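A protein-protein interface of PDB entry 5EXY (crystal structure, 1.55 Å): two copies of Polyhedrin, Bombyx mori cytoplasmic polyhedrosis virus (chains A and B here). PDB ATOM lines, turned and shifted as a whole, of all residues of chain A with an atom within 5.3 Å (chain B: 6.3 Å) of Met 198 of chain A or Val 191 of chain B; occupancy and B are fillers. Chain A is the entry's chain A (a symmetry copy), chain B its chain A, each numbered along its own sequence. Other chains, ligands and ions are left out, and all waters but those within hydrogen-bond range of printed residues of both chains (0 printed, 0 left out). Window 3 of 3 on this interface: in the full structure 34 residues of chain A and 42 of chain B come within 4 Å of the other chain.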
ATOM      1  N   ALA A 194       8.783  22.171 -18.529  1.00  0.00           N
ATOM      2  CA  ALA A 194       8.366  22.687 -19.831  1.00  0.00           C
ATOM      3  C   ALA A 194       7.659  24.012 -19.782  1.00  0.00           C
ATOM      4  O   ALA A 194       7.851  24.828 -20.668  1.00  0.00           O
ATOM      5  CB  ALA A 194       7.505  21.663 -20.554  1.00  0.00           C
ATOM      6  N   ASN A 196       8.226  26.641 -18.093  1.00  0.00           N
ATOM      7  CA  ASN A 196       9.129  27.796 -17.983  1.00  0.00           C
ATOM      8  C   ASN A 196      10.519  27.623 -18.584  1.00  0.00           C
ATOM      9  O   ASN A 196      11.284  28.583 -18.577  1.00  0.00           O
ATOM     10  CB  ASN A 196       9.240  28.182 -16.525  1.00  0.00           C
ATOM     11  CG  ASN A 196       9.826  29.542 -16.295  1.00  0.00           C
ATOM     12  OD1 ASN A 196       9.210  30.543 -16.654  1.00  0.00           O
ATOM     13  ND2 ASN A 196      10.976  29.611 -15.659  1.00  0.00           N
ATOM     14  N   VAL A 197      10.862  26.452 -19.136  1.00  0.00           N
ATOM     15  CA  VAL A 197      12.192  26.222 -19.676  1.00  0.00           C
ATOM     16  C   VAL A 197      12.663  27.241 -20.720  1.00  0.00           C
ATOM     17  O   VAL A 197      13.837  27.543 -20.718  1.00  0.00           O
ATOM     18  CB  VAL A 197      12.300  24.780 -20.234  1.00  0.00           C
ATOM     19  CG1 VAL A 197      11.452  24.621 -21.486  1.00  0.00           C
ATOM     20  CG2 VAL A 197      13.758  24.394 -20.497  1.00  0.00           C
ATOM     21  N   MET A 198      11.790  27.777 -21.619  1.00  0.00           N
ATOM     22  CA  MET A 198      12.269  28.751 -22.582  1.00  0.00           C
ATOM     23  C   MET A 198      12.650  30.063 -21.909  1.00  0.00           C
ATOM     24  O   MET A 198      13.585  30.709 -22.367  1.00  0.00           O
ATOM     25  CB  MET A 198      11.295  28.947 -23.736  1.00  0.00           C
ATOM     26  CG  MET A 198      11.146  27.707 -24.610  1.00  0.00           C
ATOM     27  SD  MET A 198      12.689  27.104 -25.300  1.00  0.00           S
ATOM     28  CE  MET A 198      13.063  28.378 -26.425  1.00  0.00           C
ATOM     29  N   ASP A 199      12.054  30.379 -20.732  1.00  0.00           N
ATOM     30  CA  ASP A 199      12.495  31.535 -19.940  1.00  0.00           C
ATOM     31  C   ASP A 199      13.886  31.290 -19.355  1.00  0.00           C
ATOM     32  O   ASP A 199      14.712  32.220 -19.278  1.00  0.00           O
ATOM     33  CB  ASP A 199      11.514  31.827 -18.800  1.00  0.00           C
ATOM     34  CG  ASP A 199      10.293  32.537 -19.328  1.00  0.00           C
ATOM     35  OD1 ASP A 199       9.722  32.053 -20.316  1.00  0.00           O
ATOM     36  OD2 ASP A 199       9.976  33.653 -18.815  1.00  0.00           O
ATOM     37  N   VAL A 200      14.202  30.021 -19.007  1.00  0.00           N
ATOM     38  CA  VAL A 200      15.559  29.731 -18.534  1.00  0.00           C
ATOM     39  C   VAL A 200      16.525  29.856 -19.698  1.00  0.00           C
ATOM     40  O   VAL A 200      17.583  30.462 -19.542  1.00  0.00           O
ATOM     41  CB  VAL A 200      15.701  28.371 -17.806  1.00  0.00           C
ATOM     42  CG1 VAL A 200      17.130  28.243 -17.219  1.00  0.00           C
ATOM     43  CG2 VAL A 200      14.667  28.275 -16.685  1.00  0.00           C
ATOM     44  N   PHE A 201      16.146  29.406 -20.904  1.00  0.00           N
ATOM     45  CA  PHE A 201      17.016  29.637 -22.079  1.00  0.00           C
ATOM     46  C   PHE A 201      17.249  31.124 -22.314  1.00  0.00           C
ATOM     47  O   PHE A 201      18.359  31.537 -22.626  1.00  0.00           O
ATOM     48  CB  PHE A 201      16.457  28.953 -23.350  1.00  0.00           C
ATOM     49  CG  PHE A 201      16.788  27.479 -23.469  1.00  0.00           C
ATOM     50  CD1 PHE A 201      18.100  27.057 -23.598  1.00  0.00           C
ATOM     51  CD2 PHE A 201      15.813  26.516 -23.277  1.00  0.00           C
ATOM     52  CE1 PHE A 201      18.407  25.705 -23.695  1.00  0.00           C
ATOM     53  CE2 PHE A 201      16.130  25.153 -23.325  1.00  0.00           C
ATOM     54  CZ  PHE A 201      17.420  24.764 -23.516  1.00  0.00           C
ATOM     55  N   GLN A 202      16.201  31.943 -22.196  1.00  0.00           N
ATOM     56  CA  GLN A 202      16.387  33.391 -22.348  1.00  0.00           C
ATOM     57  C   GLN A 202      17.277  33.939 -21.281  1.00  0.00           C
ATOM     58  O   GLN A 202      18.036  34.869 -21.564  1.00  0.00           O
ATOM     59  CB  GLN A 202      15.053  34.131 -22.338  1.00  0.00           C
ATOM     60  CG  GLN A 202      14.288  33.873 -23.623  1.00  0.00           C
ATOM     61  CD  GLN A 202      13.197  34.874 -23.818  1.00  0.00           C
ATOM     62  OE1 GLN A 202      13.382  35.924 -24.459  1.00  0.00           O
ATOM     63  NE2 GLN A 202      12.052  34.608 -23.247  1.00  0.00           N
ATOM     64  N   SER A 203      17.228  33.377 -20.050  1.00  0.00           N
ATOM     65  CA  SER A 203      18.081  33.867 -19.004  1.00  0.00           C
ATOM     66  C   SER A 203      19.551  33.678 -19.387  1.00  0.00           C
ATOM     67  O   SER A 203      20.361  34.503 -18.971  1.00  0.00           O
ATOM     68  CB  SER A 203      17.764  33.205 -17.665  1.00  0.00           C
ATOM     69  OG  SER A 203      18.337  31.917 -17.499  1.00  0.00           O
ATOM     70  N   LEU B  31       9.443  26.403 -37.375  1.00  0.00           N
ATOM     71  CA  LEU B  31      10.344  26.128 -36.243  1.00  0.00           C
ATOM     72  C   LEU B  31      11.704  25.667 -36.701  1.00  0.00           C
ATOM     73  O   LEU B  31      12.648  25.646 -35.911  1.00  0.00           O
ATOM     74  CB  LEU B  31       9.702  25.143 -35.261  1.00  0.00           C
ATOM     75  CG  LEU B  31       8.448  25.697 -34.588  1.00  0.00           C
ATOM     76  CD1 LEU B  31       7.677  24.626 -33.774  1.00  0.00           C
ATOM     77  CD2 LEU B  31       8.781  26.893 -33.767  1.00  0.00           C
ATOM     78  N   TYR B  57      15.150  28.751 -32.606  1.00  0.00           N
ATOM     79  CA  TYR B  57      14.352  28.723 -31.369  1.00  0.00           C
ATOM     80  C   TYR B  57      14.351  29.981 -30.553  1.00  0.00           C
ATOM     81  O   TYR B  57      13.290  30.403 -30.123  1.00  0.00           O
ATOM     82  CB  TYR B  57      14.753  27.559 -30.434  1.00  0.00           C
ATOM     83  CG  TYR B  57      14.807  26.225 -31.133  1.00  0.00           C
ATOM     84  CD1 TYR B  57      13.667  25.677 -31.704  1.00  0.00           C
ATOM     85  CD2 TYR B  57      15.984  25.500 -31.193  1.00  0.00           C
ATOM     86  CE1 TYR B  57      13.720  24.462 -32.392  1.00  0.00           C
ATOM     87  CE2 TYR B  57      16.042  24.261 -31.814  1.00  0.00           C
ATOM     88  CZ  TYR B  57      14.899  23.734 -32.400  1.00  0.00           C
ATOM     89  OH  TYR B  57      14.929  22.494 -32.989  1.00  0.00           O
ATOM     90  N   LYS B  58      15.531  30.474 -30.208  1.00  0.00           N
ATOM     91  CA  LYS B  58      15.674  31.674 -29.395  1.00  0.00           C
ATOM     92  C   LYS B  58      17.025  32.263 -29.688  1.00  0.00           C
ATOM     93  O   LYS B  58      17.902  31.560 -30.173  1.00  0.00           O
ATOM     94  CB  LYS B  58      15.503  31.364 -27.888  1.00  0.00           C
ATOM     95  CG  LYS B  58      16.582  30.449 -27.273  1.00  0.00           C
ATOM     96  CD  LYS B  58      17.794  31.156 -26.679  1.00  0.00           C
ATOM     97  CE  LYS B  58      18.891  30.193 -26.268  1.00  0.00           C
ATOM     98  NZ  LYS B  58      20.081  30.916 -25.720  1.00  0.00           N
ATOM     99  N   VAL B 182      12.383  35.064 -28.520  1.00  0.00           N
ATOM    100  CA  VAL B 182      12.092  33.695 -28.899  1.00  0.00           C
ATOM    101  C   VAL B 182      11.432  33.658 -30.264  1.00  0.00           C
ATOM    102  O   VAL B 182      10.606  34.496 -30.583  1.00  0.00           O
ATOM    103  CB  VAL B 182      11.176  33.073 -27.816  1.00  0.00           C
ATOM    104  CG1 VAL B 182      10.746  31.658 -28.178  1.00  0.00           C
ATOM    105  CG2 VAL B 182      11.852  33.101 -26.448  1.00  0.00           C
ATOM    106  N   ASN B 185       6.084  30.668 -32.281  1.00  0.00           N
ATOM    107  CA  ASN B 185       5.666  29.281 -32.168  1.00  0.00           C
ATOM    108  C   ASN B 185       4.183  29.269 -31.874  1.00  0.00           C
ATOM    109  O   ASN B 185       3.776  29.246 -30.701  1.00  0.00           O
ATOM    110  CB  ASN B 185       6.435  28.477 -31.150  1.00  0.00           C
ATOM    111  CG  ASN B 185       5.959  27.037 -31.179  1.00  0.00           C
ATOM    112  OD1 ASN B 185       5.184  26.656 -32.044  1.00  0.00           O
ATOM    113  ND2 ASN B 185       6.434  26.224 -30.282  1.00  0.00           N
ATOM    114  N   TYR B 189       3.357  22.555 -29.735  1.00  0.00           N
ATOM    115  CA  TYR B 189       4.565  21.749 -29.576  1.00  0.00           C
ATOM    116  C   TYR B 189       5.555  22.688 -28.927  1.00  0.00           C
ATOM    117  O   TYR B 189       6.057  23.596 -29.603  1.00  0.00           O
ATOM    118  CB  TYR B 189       5.100  21.277 -30.944  1.00  0.00           C
ATOM    119  CG  TYR B 189       6.259  20.321 -30.828  1.00  0.00           C
ATOM    120  CD1 TYR B 189       7.568  20.784 -30.796  1.00  0.00           C
ATOM    121  CD2 TYR B 189       6.046  18.956 -30.715  1.00  0.00           C
ATOM    122  CE1 TYR B 189       8.632  19.912 -30.622  1.00  0.00           C
ATOM    123  CE2 TYR B 189       7.106  18.074 -30.557  1.00  0.00           C
ATOM    124  CZ  TYR B 189       8.397  18.558 -30.509  1.00  0.00           C
ATOM    125  OH  TYR B 189       9.468  17.703 -30.428  1.00  0.00           O
ATOM    126  N   ASN B 190       5.895  22.451 -27.668  1.00  0.00           N
ATOM    127  CA  ASN B 190       6.866  23.288 -26.977  1.00  0.00           C
ATOM    128  C   ASN B 190       8.266  22.834 -27.430  1.00  0.00           C
ATOM    129  O   ASN B 190       8.632  21.668 -27.203  1.00  0.00           O
ATOM    130  CB  ASN B 190       6.689  23.107 -25.472  1.00  0.00           C
ATOM    131  CG  ASN B 190       7.630  23.921 -24.598  1.00  0.00           C
ATOM    132  OD1 ASN B 190       8.672  24.400 -25.061  1.00  0.00           O
ATOM    133  ND2 ASN B 190       7.239  24.187 -23.346  1.00  0.00           N
ATOM    134  N   VAL B 191       9.056  23.737 -28.025  1.00  0.00           N
ATOM    135  CA  VAL B 191      10.390  23.379 -28.520  1.00  0.00           C
ATOM    136  C   VAL B 191      11.338  23.028 -27.405  1.00  0.00           C
ATOM    137  O   VAL B 191      12.323  22.323 -27.649  1.00  0.00           O
ATOM    138  CB  VAL B 191      11.008  24.430 -29.475  1.00  0.00           C
ATOM    139  CG1 VAL B 191      10.137  24.635 -30.722  1.00  0.00           C
ATOM    140  CG2 VAL B 191      11.319  25.745 -28.773  1.00  0.00           C
ATOM    141  N   GLY B 192      11.012  23.460 -26.187  1.00  0.00           N
ATOM    142  CA  GLY B 192      11.794  23.176 -24.990  1.00  0.00           C
ATOM    143  C   GLY B 192      11.231  22.075 -24.125  1.00  0.00           C
ATOM    144  O   GLY B 192      11.831  21.780 -23.094  1.00  0.00           O
ATOM    145  N   SER B 193      10.146  21.406 -24.547  1.00  0.00           N
ATOM    146  CA  SER B 193       9.679  20.243 -23.809  1.00  0.00           C
ATOM    147  C   SER B 193      10.694  19.127 -24.009  1.00  0.00           C
ATOM    148  O   SER B 193      11.611  19.258 -24.818  1.00  0.00           O
ATOM    149  CB  SER B 193       8.293  19.813 -24.259  1.00  0.00           C
ATOM    150  OG  SER B 193       8.264  19.480 -25.631  1.00  0.00           O
ATOM    151  N   HIS B 195      10.945  16.274 -25.419  1.00  0.00           N
ATOM    152  CA  HIS B 195      11.274  15.690 -26.694  1.00  0.00           C
ATOM    153  C   HIS B 195      12.345  16.449 -27.408  1.00  0.00           C
ATOM    154  O   HIS B 195      13.267  15.824 -27.903  1.00  0.00           O
ATOM    155  CB  HIS B 195      10.033  15.593 -27.599  1.00  0.00           C
ATOM    156  CG  HIS B 195       9.182  14.403 -27.376  1.00  0.00           C
ATOM    157  ND1 HIS B 195       9.204  13.712 -26.195  1.00  0.00           N
ATOM    158  CD2 HIS B 195       8.226  13.871 -28.172  1.00  0.00           C
ATOM    159  CE1 HIS B 195       8.240  12.817 -26.293  1.00  0.00           C
ATOM    160  NE2 HIS B 195       7.730  12.778 -27.512  1.00  0.00           N
ATOM    161  N   ASN B 196      12.291  17.772 -27.403  1.00  0.00           N
ATOM    162  CA  ASN B 196      13.207  18.591 -28.209  1.00  0.00           C
ATOM    163  C   ASN B 196      14.184  19.469 -27.435  1.00  0.00           C
ATOM    164  O   ASN B 196      15.013  20.119 -28.064  1.00  0.00           O
ATOM    165  CB  ASN B 196      12.387  19.440 -29.155  1.00  0.00           C
ATOM    166  CG  ASN B 196      13.178  20.048 -30.273  1.00  0.00           C
ATOM    167  OD1 ASN B 196      13.676  19.327 -31.134  1.00  0.00           O
ATOM    168  ND2 ASN B 196      13.264  21.361 -30.314  1.00  0.00           N
ATOM    169  N   VAL B 197      14.142  19.486 -26.096  1.00  0.00           N
ATOM    170  CA  VAL B 197      15.018  20.345 -25.315  1.00  0.00           C
ATOM    171  C   VAL B 197      16.515  20.197 -25.609  1.00  0.00           C
ATOM    172  O   VAL B 197      17.196  21.199 -25.564  1.00  0.00           O
ATOM    173  CB  VAL B 197      14.737  20.159 -23.802  1.00  0.00           C
ATOM    174  CG1 VAL B 197      15.192  18.786 -23.333  1.00  0.00           C
ATOM    175  CG2 VAL B 197      15.387  21.272 -22.976  1.00  0.00           C
ATOM    176  N   MET B 198      17.056  18.980 -25.898  1.00  0.00           N
ATOM    177  CA  MET B 198      18.475  18.882 -26.186  1.00  0.00           C
ATOM    178  C   MET B 198      18.825  19.546 -27.511  1.00  0.00           C
ATOM    179  O   MET B 198      19.911  20.102 -27.622  1.00  0.00           O
ATOM    180  CB  MET B 198      18.983  17.450 -26.098  1.00  0.00           C
ATOM    181  CG  MET B 198      18.922  16.879 -24.686  1.00  0.00           C
ATOM    182  SD  MET B 198      19.812  17.845 -23.463  1.00  0.00           S
ATOM    183  CE  MET B 198      21.455  17.571 -23.965  1.00  0.00           C
ATOM    184  N   ASP B 199      17.856  19.645 -28.457  1.00  0.00           N
ATOM    185  CA  ASP B 199      18.066  20.423 -29.685  1.00  0.00           C
ATOM    186  C   ASP B 199      18.137  21.918 -29.372  1.00  0.00           C
ATOM    187  O   ASP B 199      18.927  22.657 -29.990  1.00  0.00           O
ATOM    188  CB  ASP B 199      16.939  20.174 -30.693  1.00  0.00           C
ATOM    189  CG  ASP B 199      17.141  18.850 -31.387  1.00  0.00           C
ATOM    190  OD1 ASP B 199      17.361  17.853 -30.684  1.00  0.00           O
ATOM    191  OD2 ASP B 199      17.194  18.836 -32.654  1.00  0.00           O
ATOM    192  N   VAL B 200      17.375  22.378 -28.353  1.00  0.00           N
ATOM    193  CA  VAL B 200      17.490  23.786 -27.960  1.00  0.00           C
ATOM    194  C   VAL B 200      18.840  24.007 -27.304  1.00  0.00           C
ATOM    195  O   VAL B 200      19.511  24.988 -27.619  1.00  0.00           O
ATOM    196  CB  VAL B 200      16.324  24.297 -27.076  1.00  0.00           C
ATOM    197  CG1 VAL B 200      16.471  25.824 -26.854  1.00  0.00           C
ATOM    198  CG2 VAL B 200      14.989  23.995 -27.756  1.00  0.00           C
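Of chain B, only Val 191 comes within 4 Å of Met 198 of chain A.
Printed residues of chain B within 4 Å of Phe 201 of chain A: Lys 58, Val 197 and Val 200.
Of the printed residues of chain A, Lys 58 of chain B touches Phe 201.
Of the printed residues of chain A, Val 182 of chain B touches Gln 202 (3.4 Å).
Of the printed residues of chain A, Val 191 of chain B touches Met 198 (3.9 Å).
Of the printed residues of chain A, Val 197 of chain B touches Phe 201.
Printed residues of chain A within 4 Å of Val 200 of chain B: Phe 201 (3.6 Å).
The nearest residue of chain B that does not touch Met 198 of chain A is Gly 192 of chain B (4.04 Å).
O of Ala 194 of chain A lies within hydrogen-bond range of ND2 of Asn 190 of chain B (2.8 Å).
N of Gly 192 of chain B is in hydrogen-bond range of OD1 of Asn 190 of chain B, at 2.8 Å.
O of Val 191 of chain B is in hydrogen-bond range of ND2 of Asn 196 of chain B (3.0 Å).
The backbone carbonyl oxygen (O) of Asn 190 of chain B sits at hydrogen-bond distance from the side-chain hydroxyl (OG) of Ser 193 of chain B, at 2.7 Å.
5 positions are printed for both chains.
Of the 16 printed residues of chain B, 7 touch a printed residue of chain A.
Among the printed residues, 7 pairs touch across the chains.
Among the printed residues, no Asp or Glu carboxylate lies within 4 Å of a Lys or Arg side-chain nitrogen of the other chain.
Among the printed residues, pairs that only touch across the chains: Val 197 of chain A with Gly 192 of chain B (3.3 Å), Met 198 of chain A with Val 191 of chain B (3.9 Å), Phe 201 of chain A with Lys 58 of chain B (3.6 Å), Phe 201 of chain A with Val 197 of chain B (3.97 Å), Phe 201 of chain A with Val 200 of chain B (3.6 Å) and Gln 202 of chain A with Val 182 of chain B (3.4 Å).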
